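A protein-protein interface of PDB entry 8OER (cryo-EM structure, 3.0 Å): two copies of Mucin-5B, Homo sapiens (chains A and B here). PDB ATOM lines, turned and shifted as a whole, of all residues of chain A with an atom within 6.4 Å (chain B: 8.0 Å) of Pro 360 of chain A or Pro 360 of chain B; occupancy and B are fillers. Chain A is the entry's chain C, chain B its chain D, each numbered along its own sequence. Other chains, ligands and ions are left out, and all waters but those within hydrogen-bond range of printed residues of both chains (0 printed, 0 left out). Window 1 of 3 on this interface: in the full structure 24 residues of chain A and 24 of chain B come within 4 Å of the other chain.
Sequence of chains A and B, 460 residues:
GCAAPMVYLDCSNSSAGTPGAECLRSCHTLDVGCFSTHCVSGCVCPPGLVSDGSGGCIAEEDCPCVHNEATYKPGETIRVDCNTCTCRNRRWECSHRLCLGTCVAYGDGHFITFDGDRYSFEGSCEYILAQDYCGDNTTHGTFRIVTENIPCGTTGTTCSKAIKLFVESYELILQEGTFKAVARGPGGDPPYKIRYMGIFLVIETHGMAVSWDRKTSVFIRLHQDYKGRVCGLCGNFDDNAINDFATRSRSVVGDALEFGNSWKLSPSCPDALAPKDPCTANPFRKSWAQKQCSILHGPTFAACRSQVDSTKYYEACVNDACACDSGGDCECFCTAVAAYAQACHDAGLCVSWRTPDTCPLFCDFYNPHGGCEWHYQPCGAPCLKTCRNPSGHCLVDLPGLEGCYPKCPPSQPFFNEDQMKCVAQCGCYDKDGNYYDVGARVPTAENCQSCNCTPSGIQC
Among the printed residues, merely in contact across the chains: Leu 361 of chain A with Phe 362 of chain B, Phe 362 of chain A with Leu 361 of chain B, Phe 362 of chain A with Arg 354 of chain B, Phe 362 of chain A with Pro 360 of chain B, Pro 360 of chain A with Phe 362 of chain B, Arg 354 of chain A with Phe 362 of chain B, Pro 356 of chain A with Phe 362 of chain B, Pro 360 of chain A with Pro 360 of chain B, Phe 362 of chain A with Pro 356 of chain B and Phe 362 of chain A with Tyr 376 of chain B.
Printed residues of chain B that touch a printed residue of chain A: Arg 354, Pro 356, Pro 360, Leu 361, Phe 362 and Tyr 376.
Hydrophobic or aromatic side chains of chain B that line the printed part of chain A: Pro 356, Pro 360, Phe 362 and Tyr 376.
Hydrophobic or aromatic side chains of chain A that line the printed part of chain B: Pro 356, Pro 360 and Phe 362.
Among the printed residues, 10 pairs touch across the chains.
Among the printed residues, no Asp or Glu carboxylate lies within 4 Å of a Lys or Arg side-chain nitrogen of the other chain.
O of Cys 359 of chain A lies within hydrogen-bond range of NH1 of Arg 354 of chain A, at 3.2 Å.
OH of Tyr 376 of chain B lies close to NE of Arg 354 of chain B, 3.1 Å away.
The guanidinium group (NH1) of Arg 354 of chain B lies within hydrogen-bond range of the backbone carbonyl oxygen (O) of Cys 359 of chain B (3.1 Å).
The side-chain sulfur (SG) of Cys 334 of chain A forms a disulfide with the side-chain sulfur (SG) of Cys 359 of chain A (2.0 Å).
SG of Cys 359 of chain B is disulfide-bonded to SG of Cys 334 of chain B, 2.0 Å away.
Of chain B, only Pro 360 (3.8 Å) and Phe 362 (3.5 Å) come within 4 Å of Pro 360 of chain A.
Of chain A, only Pro 360 (3.8 Å) and Phe 362 (3.5 Å) come within 4 Å of Pro 360 of chain B.
Printed residues of chain B within 4 Å of Phe 362 of chain A: Arg 354 (3.4 Å), Pro 356 (3.9 Å), Pro 360 (3.5 Å), Leu 361 (3.2 Å) and Tyr 376 (3.9 Å).
Of the printed residues of chain A, Tyr 376 of chain B touches Phe 362 (3.9 Å).
Of the printed residues of chain A, Leu 361 of chain B touches Phe 362 (3.2 Å).
The nearest residue of chain B that does not touch Pro 360 of chain A is Leu 361 of chain B (4.6 Å).
The nearest residue of chain A that does not touch Pro 360 of chain B is Leu 361 of chain A (4.5 Å).
Pro 356 of chain A touches Phe 362 of chain B, and with the chains exchanged Phe 362 of chain A touches Pro 356 of chain B.
Pro 360 of chain A touches its own counterpart, Pro 360 of chain B.
Pro 360 of chain A touches Phe 362 of chain B, and with the chains exchanged Phe 362 of chain A touches Pro 360 of chain B.
Leu 361 of chain A touches Phe 362 of chain B, and with the chains exchanged Phe 362 of chain A touches Leu 361 of chain B.
Of the 10 pairs that touch across the chains among the printed residues, 9 have their exchanged pair printed and touching as well.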
ATOM      1  N   CYS A 334      -8.878  12.533  -6.527  1.00  0.00           N
ATOM      2  CA  CYS A 334      -9.683  11.358  -6.230  1.00  0.00           C
ATOM      3  C   CYS A 334     -10.520  10.951  -7.427  1.00  0.00           C
ATOM      4  O   CYS A 334     -10.581   9.771  -7.776  1.00  0.00           O
ATOM      5  CB  CYS A 334     -10.587  11.626  -5.030  1.00  0.00           C
ATOM      6  SG  CYS A 334      -9.808  11.493  -3.416  1.00  0.00           S
ATOM      7  N   ARG A 354      -7.832   3.388  -2.373  1.00  0.00           N
ATOM      8  CA  ARG A 354      -8.583   4.040  -1.300  1.00  0.00           C
ATOM      9  C   ARG A 354      -8.004   3.873   0.100  1.00  0.00           C
ATOM     10  O   ARG A 354      -8.726   3.478   1.015  1.00  0.00           O
ATOM     11  CB  ARG A 354     -10.034   3.574  -1.327  1.00  0.00           C
ATOM     12  CG  ARG A 354     -10.851   4.256  -2.419  1.00  0.00           C
ATOM     13  CD  ARG A 354     -12.040   4.996  -1.857  1.00  0.00           C
ATOM     14  NE  ARG A 354     -12.912   5.499  -2.908  1.00  0.00           N
ATOM     15  CZ  ARG A 354     -12.845   6.722  -3.412  1.00  0.00           C
ATOM     16  NH1 ARG A 354     -11.951   7.596  -2.989  1.00  0.00           N
ATOM     17  NH2 ARG A 354     -13.698   7.078  -4.365  1.00  0.00           N
ATOM     18  N   THR A 355      -6.728   4.159   0.291  1.00  0.00           N
ATOM     19  CA  THR A 355      -6.137   3.991   1.608  1.00  0.00           C
ATOM     20  C   THR A 355      -6.513   5.155   2.513  1.00  0.00           C
ATOM     21  O   THR A 355      -6.924   6.209   2.036  1.00  0.00           O
ATOM     22  CB  THR A 355      -4.625   3.886   1.495  1.00  0.00           C
ATOM     23  OG1 THR A 355      -4.145   4.877   0.582  1.00  0.00           O
ATOM     24  CG2 THR A 355      -4.224   2.514   1.004  1.00  0.00           C
ATOM     25  N   PRO A 356      -6.396   4.984   3.831  1.00  0.00           N
ATOM     26  CA  PRO A 356      -6.711   6.098   4.738  1.00  0.00           C
ATOM     27  C   PRO A 356      -5.896   7.348   4.474  1.00  0.00           C
ATOM     28  O   PRO A 356      -6.375   8.458   4.728  1.00  0.00           O
ATOM     29  CB  PRO A 356      -6.411   5.513   6.120  1.00  0.00           C
ATOM     30  CG  PRO A 356      -6.635   4.064   5.959  1.00  0.00           C
ATOM     31  CD  PRO A 356      -6.239   3.713   4.557  1.00  0.00           C
ATOM     32  N   ASP A 357      -4.671   7.203   3.987  1.00  0.00           N
ATOM     33  CA  ASP A 357      -3.882   8.356   3.585  1.00  0.00           C
ATOM     34  C   ASP A 357      -4.315   8.923   2.242  1.00  0.00           C
ATOM     35  O   ASP A 357      -4.159  10.125   2.015  1.00  0.00           O
ATOM     36  CB  ASP A 357      -2.401   7.979   3.519  1.00  0.00           C
ATOM     37  CG  ASP A 357      -1.635   8.390   4.757  1.00  0.00           C
ATOM     38  OD1 ASP A 357      -1.722   9.572   5.146  1.00  0.00           O
ATOM     39  OD2 ASP A 357      -0.945   7.532   5.341  1.00  0.00           O
ATOM     40  N   THR A 358      -4.855   8.093   1.357  1.00  0.00           N
ATOM     41  CA  THR A 358      -5.100   8.466  -0.032  1.00  0.00           C
ATOM     42  C   THR A 358      -6.573   8.270  -0.357  1.00  0.00           C
ATOM     43  O   THR A 358      -7.045   7.133  -0.425  1.00  0.00           O
ATOM     44  CB  THR A 358      -4.243   7.628  -0.973  1.00  0.00           C
ATOM     45  OG1 THR A 358      -2.862   7.940  -0.765  1.00  0.00           O
ATOM     46  CG2 THR A 358      -4.623   7.887  -2.417  1.00  0.00           C
ATOM     47  N   CYS A 359      -7.283   9.368  -0.588  1.00  0.00           N
ATOM     48  CA  CYS A 359      -8.693   9.337  -0.958  1.00  0.00           C
ATOM     49  C   CYS A 359      -9.509   8.472   0.002  1.00  0.00           C
ATOM     50  O   CYS A 359     -10.056   7.439  -0.398  1.00  0.00           O
ATOM     51  CB  CYS A 359      -8.864   8.851  -2.389  1.00  0.00           C
ATOM     52  SG  CYS A 359      -8.409  10.048  -3.638  1.00  0.00           S
ATOM     53  N   PRO A 360      -9.593   8.847   1.271  1.00  0.00           N
ATOM     54  CA  PRO A 360     -10.397   8.067   2.206  1.00  0.00           C
ATOM     55  C   PRO A 360     -11.874   8.282   1.942  1.00  0.00           C
ATOM     56  O   PRO A 360     -12.294   9.292   1.378  1.00  0.00           O
ATOM     57  CB  PRO A 360      -9.987   8.620   3.569  1.00  0.00           C
ATOM     58  CG  PRO A 360      -9.592  10.010   3.297  1.00  0.00           C
ATOM     59  CD  PRO A 360      -9.147  10.115   1.864  1.00  0.00           C
ATOM     60  N   LEU A 361     -12.667   7.302   2.349  1.00  0.00           N
ATOM     61  CA  LEU A 361     -14.116   7.358   2.192  1.00  0.00           C
ATOM     62  C   LEU A 361     -14.755   7.022   3.527  1.00  0.00           C
ATOM     63  O   LEU A 361     -14.742   5.863   3.950  1.00  0.00           O
ATOM     64  CB  LEU A 361     -14.594   6.396   1.111  1.00  0.00           C
ATOM     65  CG  LEU A 361     -15.622   6.971   0.143  1.00  0.00           C
ATOM     66  CD1 LEU A 361     -15.045   8.157  -0.615  1.00  0.00           C
ATOM     67  CD2 LEU A 361     -16.076   5.887  -0.803  1.00  0.00           C
ATOM     68  N   PHE A 362     -15.312   8.029   4.187  1.00  0.00           N
ATOM     69  CA  PHE A 362     -15.978   7.807   5.461  1.00  0.00           C
ATOM     70  C   PHE A 362     -17.196   6.934   5.229  1.00  0.00           C
ATOM     71  O   PHE A 362     -18.125   7.332   4.525  1.00  0.00           O
ATOM     72  CB  PHE A 362     -16.373   9.135   6.091  1.00  0.00           C
ATOM     73  CG  PHE A 362     -16.450   9.092   7.577  1.00  0.00           C
ATOM     74  CD1 PHE A 362     -17.277   8.193   8.214  1.00  0.00           C
ATOM     75  CD2 PHE A 362     -15.690   9.947   8.340  1.00  0.00           C
ATOM     76  CE1 PHE A 362     -17.348   8.150   9.586  1.00  0.00           C
ATOM     77  CE2 PHE A 362     -15.759   9.908   9.708  1.00  0.00           C
ATOM     78  CZ  PHE A 362     -16.590   9.008  10.332  1.00  0.00           C
ATOM     79  N   LYS B 215       0.411  13.971  10.891  1.00  0.00           N
ATOM     80  CA  LYS B 215       0.669  14.891   9.791  1.00  0.00           C
ATOM     81  C   LYS B 215       1.274  16.197  10.283  1.00  0.00           C
ATOM     82  O   LYS B 215       2.451  16.436  10.032  1.00  0.00           O
ATOM     83  CB  LYS B 215      -0.618  15.144   9.003  1.00  0.00           C
ATOM     84  CG  LYS B 215      -1.518  13.928   8.870  1.00  0.00           C
ATOM     85  CD  LYS B 215      -2.385  14.004   7.629  1.00  0.00           C
ATOM     86  CE  LYS B 215      -3.855  13.862   7.970  1.00  0.00           C
ATOM     87  NZ  LYS B 215      -4.720  14.547   6.971  1.00  0.00           N
ATOM     88  N   CYS B 330      -7.235  19.811   1.469  1.00  0.00           N
ATOM     89  CA  CYS B 330      -8.142  19.246   2.452  1.00  0.00           C
ATOM     90  C   CYS B 330      -7.410  18.935   3.739  1.00  0.00           C
ATOM     91  O   CYS B 330      -7.977  19.065   4.819  1.00  0.00           O
ATOM     92  CB  CYS B 330      -8.810  17.993   1.906  1.00  0.00           C
ATOM     93  SG  CYS B 330      -9.060  18.040   0.140  1.00  0.00           S
ATOM     94  N   PHE B 333      -7.128  22.320   5.723  1.00  0.00           N
ATOM     95  CA  PHE B 333      -8.397  22.673   6.347  1.00  0.00           C
ATOM     96  C   PHE B 333      -8.765  21.682   7.446  1.00  0.00           C
ATOM     97  O   PHE B 333      -9.241  22.077   8.518  1.00  0.00           O
ATOM     98  CB  PHE B 333      -9.484  22.754   5.280  1.00  0.00           C
ATOM     99  CG  PHE B 333     -10.848  22.404   5.772  1.00  0.00           C
ATOM    100  CD1 PHE B 333     -11.580  23.301   6.514  1.00  0.00           C
ATOM    101  CD2 PHE B 333     -11.409  21.179   5.476  1.00  0.00           C
ATOM    102  CE1 PHE B 333     -12.837  22.976   6.959  1.00  0.00           C
ATOM    103  CE2 PHE B 333     -12.664  20.855   5.920  1.00  0.00           C
ATOM    104  CZ  PHE B 333     -13.378  21.754   6.663  1.00  0.00           C
ATOM    105  N   CYS B 334      -8.526  20.391   7.206  1.00  0.00           N
ATOM    106  CA  CYS B 334      -8.868  19.358   8.170  1.00  0.00           C
ATOM    107  C   CYS B 334      -8.128  19.561   9.476  1.00  0.00           C
ATOM    108  O   CYS B 334      -8.726  19.496  10.551  1.00  0.00           O
ATOM    109  CB  CYS B 334      -8.541  17.980   7.601  1.00  0.00           C
ATOM    110  SG  CYS B 334      -9.769  17.260   6.507  1.00  0.00           S
ATOM    111  N   TRP B 353     -17.724  16.204  13.979  1.00  0.00           N
ATOM    112  CA  TRP B 353     -18.040  16.891  12.737  1.00  0.00           C
ATOM    113  C   TRP B 353     -17.911  16.003  11.502  1.00  0.00           C
ATOM    114  O   TRP B 353     -18.922  15.563  10.950  1.00  0.00           O
ATOM    115  CB  TRP B 353     -17.119  18.102  12.605  1.00  0.00           C
ATOM    116  CG  TRP B 353     -15.688  17.826  13.012  1.00  0.00           C
ATOM    117  CD1 TRP B 353     -15.239  17.404  14.232  1.00  0.00           C
ATOM    118  CD2 TRP B 353     -14.524  17.979  12.199  1.00  0.00           C
ATOM    119  NE1 TRP B 353     -13.880  17.267  14.220  1.00  0.00           N
ATOM    120  CE2 TRP B 353     -13.415  17.623  12.984  1.00  0.00           C
ATOM    121  CE3 TRP B 353     -14.313  18.383  10.882  1.00  0.00           C
ATOM    122  CZ2 TRP B 353     -12.122  17.657  12.496  1.00  0.00           C
ATOM    123  CZ3 TRP B 353     -13.031  18.414  10.403  1.00  0.00           C
ATOM    124  CH2 TRP B 353     -11.950  18.057  11.205  1.00  0.00           C
ATOM    125  N   ARG B 354     -16.675  15.768  11.049  1.00  0.00           N
ATOM    126  CA  ARG B 354     -16.225  14.649  10.218  1.00  0.00           C
ATOM    127  C   ARG B 354     -17.265  14.053   9.273  1.00  0.00           C
ATOM    128  O   ARG B 354     -17.441  12.834   9.248  1.00  0.00           O
ATOM    129  CB  ARG B 354     -15.640  13.562  11.113  1.00  0.00           C
ATOM    130  CG  ARG B 354     -14.286  13.962  11.678  1.00  0.00           C
ATOM    131  CD  ARG B 354     -13.193  13.023  11.255  1.00  0.00           C
ATOM    132  NE  ARG B 354     -11.919  13.401  11.845  1.00  0.00           N
ATOM    133  CZ  ARG B 354     -11.027  14.175  11.246  1.00  0.00           C
ATOM    134  NH1 ARG B 354     -11.237  14.658  10.037  1.00  0.00           N
ATOM    135  NH2 ARG B 354      -9.895  14.466  11.874  1.00  0.00           N
ATOM    136  N   THR B 355     -17.936  14.872   8.486  1.00  0.00           N
ATOM    137  CA  THR B 355     -18.941  14.369   7.567  1.00  0.00           C
ATOM    138  C   THR B 355     -18.259  13.748   6.354  1.00  0.00           C
ATOM    139  O   THR B 355     -17.158  14.151   5.988  1.00  0.00           O
ATOM    140  CB  THR B 355     -19.855  15.513   7.146  1.00  0.00           C
ATOM    141  OG1 THR B 355     -20.216  16.272   8.303  1.00  0.00           O
ATOM    142  CG2 THR B 355     -21.129  15.004   6.506  1.00  0.00           C
ATOM    143  N   PRO B 356     -18.879  12.752   5.714  1.00  0.00           N
ATOM    144  CA  PRO B 356     -18.260  12.179   4.508  1.00  0.00           C
ATOM    145  C   PRO B 356     -17.944  13.204   3.441  1.00  0.00           C
ATOM    146  O   PRO B 356     -17.026  12.994   2.641  1.00  0.00           O
ATOM    147  CB  PRO B 356     -19.310  11.173   4.032  1.00  0.00           C
ATOM    148  CG  PRO B 356     -19.951  10.725   5.271  1.00  0.00           C
ATOM    149  CD  PRO B 356     -19.951  11.885   6.224  1.00  0.00           C
ATOM    150  N   ASP B 357     -18.684  14.304   3.398  1.00  0.00           N
ATOM    151  CA  ASP B 357     -18.344  15.410   2.518  1.00  0.00           C
ATOM    152  C   ASP B 357     -17.169  16.221   3.036  1.00  0.00           C
ATOM    153  O   ASP B 357     -16.471  16.852   2.238  1.00  0.00           O
ATOM    154  CB  ASP B 357     -19.553  16.332   2.350  1.00  0.00           C
ATOM    155  CG  ASP B 357     -20.379  15.996   1.131  1.00  0.00           C
ATOM    156  OD1 ASP B 357     -19.801  15.877   0.034  1.00  0.00           O
ATOM    157  OD2 ASP B 357     -21.609  15.852   1.269  1.00  0.00           O
ATOM    158  N   THR B 358     -16.935  16.213   4.343  1.00  0.00           N
ATOM    159  CA  THR B 358     -16.021  17.145   4.994  1.00  0.00           C
ATOM    160  C   THR B 358     -15.071  16.377   5.899  1.00  0.00           C
ATOM    161  O   THR B 358     -15.478  15.891   6.959  1.00  0.00           O
ATOM    162  CB  THR B 358     -16.800  18.180   5.801  1.00  0.00           C
ATOM    163  OG1 THR B 358     -17.497  19.057   4.908  1.00  0.00           O
ATOM    164  CG2 THR B 358     -15.870  18.982   6.690  1.00  0.00           C
ATOM    165  N   CYS B 359     -13.806  16.292   5.502  1.00  0.00           N
ATOM    166  CA  CYS B 359     -12.770  15.633   6.288  1.00  0.00           C
ATOM    167  C   CYS B 359     -13.162  14.203   6.665  1.00  0.00           C
ATOM    168  O   CYS B 359     -13.298  13.884   7.849  1.00  0.00           O
ATOM    169  CB  CYS B 359     -12.448  16.443   7.537  1.00  0.00           C
ATOM    170  SG  CYS B 359     -11.532  17.943   7.223  1.00  0.00           S
ATOM    171  N   PRO B 360     -13.356  13.327   5.687  1.00  0.00           N
ATOM    172  CA  PRO B 360     -13.673  11.939   6.007  1.00  0.00           C
ATOM    173  C   PRO B 360     -12.449  11.224   6.546  1.00  0.00           C
ATOM    174  O   PRO B 360     -11.308  11.636   6.336  1.00  0.00           O
ATOM    175  CB  PRO B 360     -14.115  11.359   4.665  1.00  0.00           C
ATOM    176  CG  PRO B 360     -13.412  12.171   3.661  1.00  0.00           C
ATOM    177  CD  PRO B 360     -13.112  13.517   4.249  1.00  0.00           C
ATOM    178  N   LEU B 361     -12.702  10.136   7.265  1.00  0.00           N
ATOM    179  CA  LEU B 361     -11.642   9.361   7.896  1.00  0.00           C
ATOM    180  C   LEU B 361     -11.912   7.885   7.664  1.00  0.00           C
ATOM    181  O   LEU B 361     -12.749   7.292   8.350  1.00  0.00           O
ATOM    182  CB  LEU B 361     -11.550   9.664   9.386  1.00  0.00           C
ATOM    183  CG  LEU B 361     -10.134   9.898   9.890  1.00  0.00           C
ATOM    184  CD1 LEU B 361      -9.499  11.051   9.134  1.00  0.00           C
ATOM    185  CD2 LEU B 361     -10.167  10.176  11.370  1.00  0.00           C
ATOM    186  N   PHE B 362     -11.199   7.293   6.717  1.00  0.00           N
ATOM    187  CA  PHE B 362     -11.425   5.901   6.355  1.00  0.00           C
ATOM    188  C   PHE B 362     -11.059   5.018   7.532  1.00  0.00           C
ATOM    189  O   PHE B 362      -9.881   4.847   7.848  1.00  0.00           O
ATOM    190  CB  PHE B 362     -10.597   5.545   5.129  1.00  0.00           C
ATOM    191  CG  PHE B 362     -11.116   4.377   4.362  1.00  0.00           C
ATOM    192  CD1 PHE B 362     -11.181   3.127   4.938  1.00  0.00           C
ATOM    193  CD2 PHE B 362     -11.547   4.528   3.066  1.00  0.00           C
ATOM    194  CE1 PHE B 362     -11.660   2.045   4.230  1.00  0.00           C
ATOM    195  CE2 PHE B 362     -12.025   3.457   2.361  1.00  0.00           C
ATOM    196  CZ  PHE B 362     -12.080   2.213   2.943  1.00  0.00           C
ATOM    197  N   CYS B 363     -12.064   4.464   8.192  1.00  0.00           N
ATOM    198  CA  CYS B 363     -11.844   3.589   9.330  1.00  0.00           C
ATOM    199  C   CYS B 363     -12.369   2.182   9.098  1.00  0.00           C
ATOM    200  O   CYS B 363     -12.179   1.311   9.954  1.00  0.00           O
ATOM    201  CB  CYS B 363     -12.473   4.190  10.589  1.00  0.00           C
ATOM    202  SG  CYS B 363     -11.529   5.596  11.149  1.00  0.00           S
ATOM    203  N   TYR B 376     -15.330   4.299  14.461  1.00  0.00           N
ATOM    204  CA  TYR B 376     -14.870   5.665  14.679  1.00  0.00           C
ATOM    205  C   TYR B 376     -15.521   6.203  15.942  1.00  0.00           C
ATOM    206  O   TYR B 376     -16.750   6.249  16.042  1.00  0.00           O
ATOM    207  CB  TYR B 376     -15.197   6.547  13.478  1.00  0.00           C
ATOM    208  CG  TYR B 376     -14.738   7.978  13.636  1.00  0.00           C
ATOM    209  CD1 TYR B 376     -15.471   8.879  14.388  1.00  0.00           C
ATOM    210  CD2 TYR B 376     -13.580   8.427  13.030  1.00  0.00           C
ATOM    211  CE1 TYR B 376     -15.060  10.172  14.543  1.00  0.00           C
ATOM    212  CE2 TYR B 376     -13.166   9.725  13.177  1.00  0.00           C
ATOM    213  CZ  TYR B 376     -13.911  10.592  13.938  1.00  0.00           C
ATOM    214  OH  TYR B 376     -13.514  11.895  14.105  1.00  0.00           O
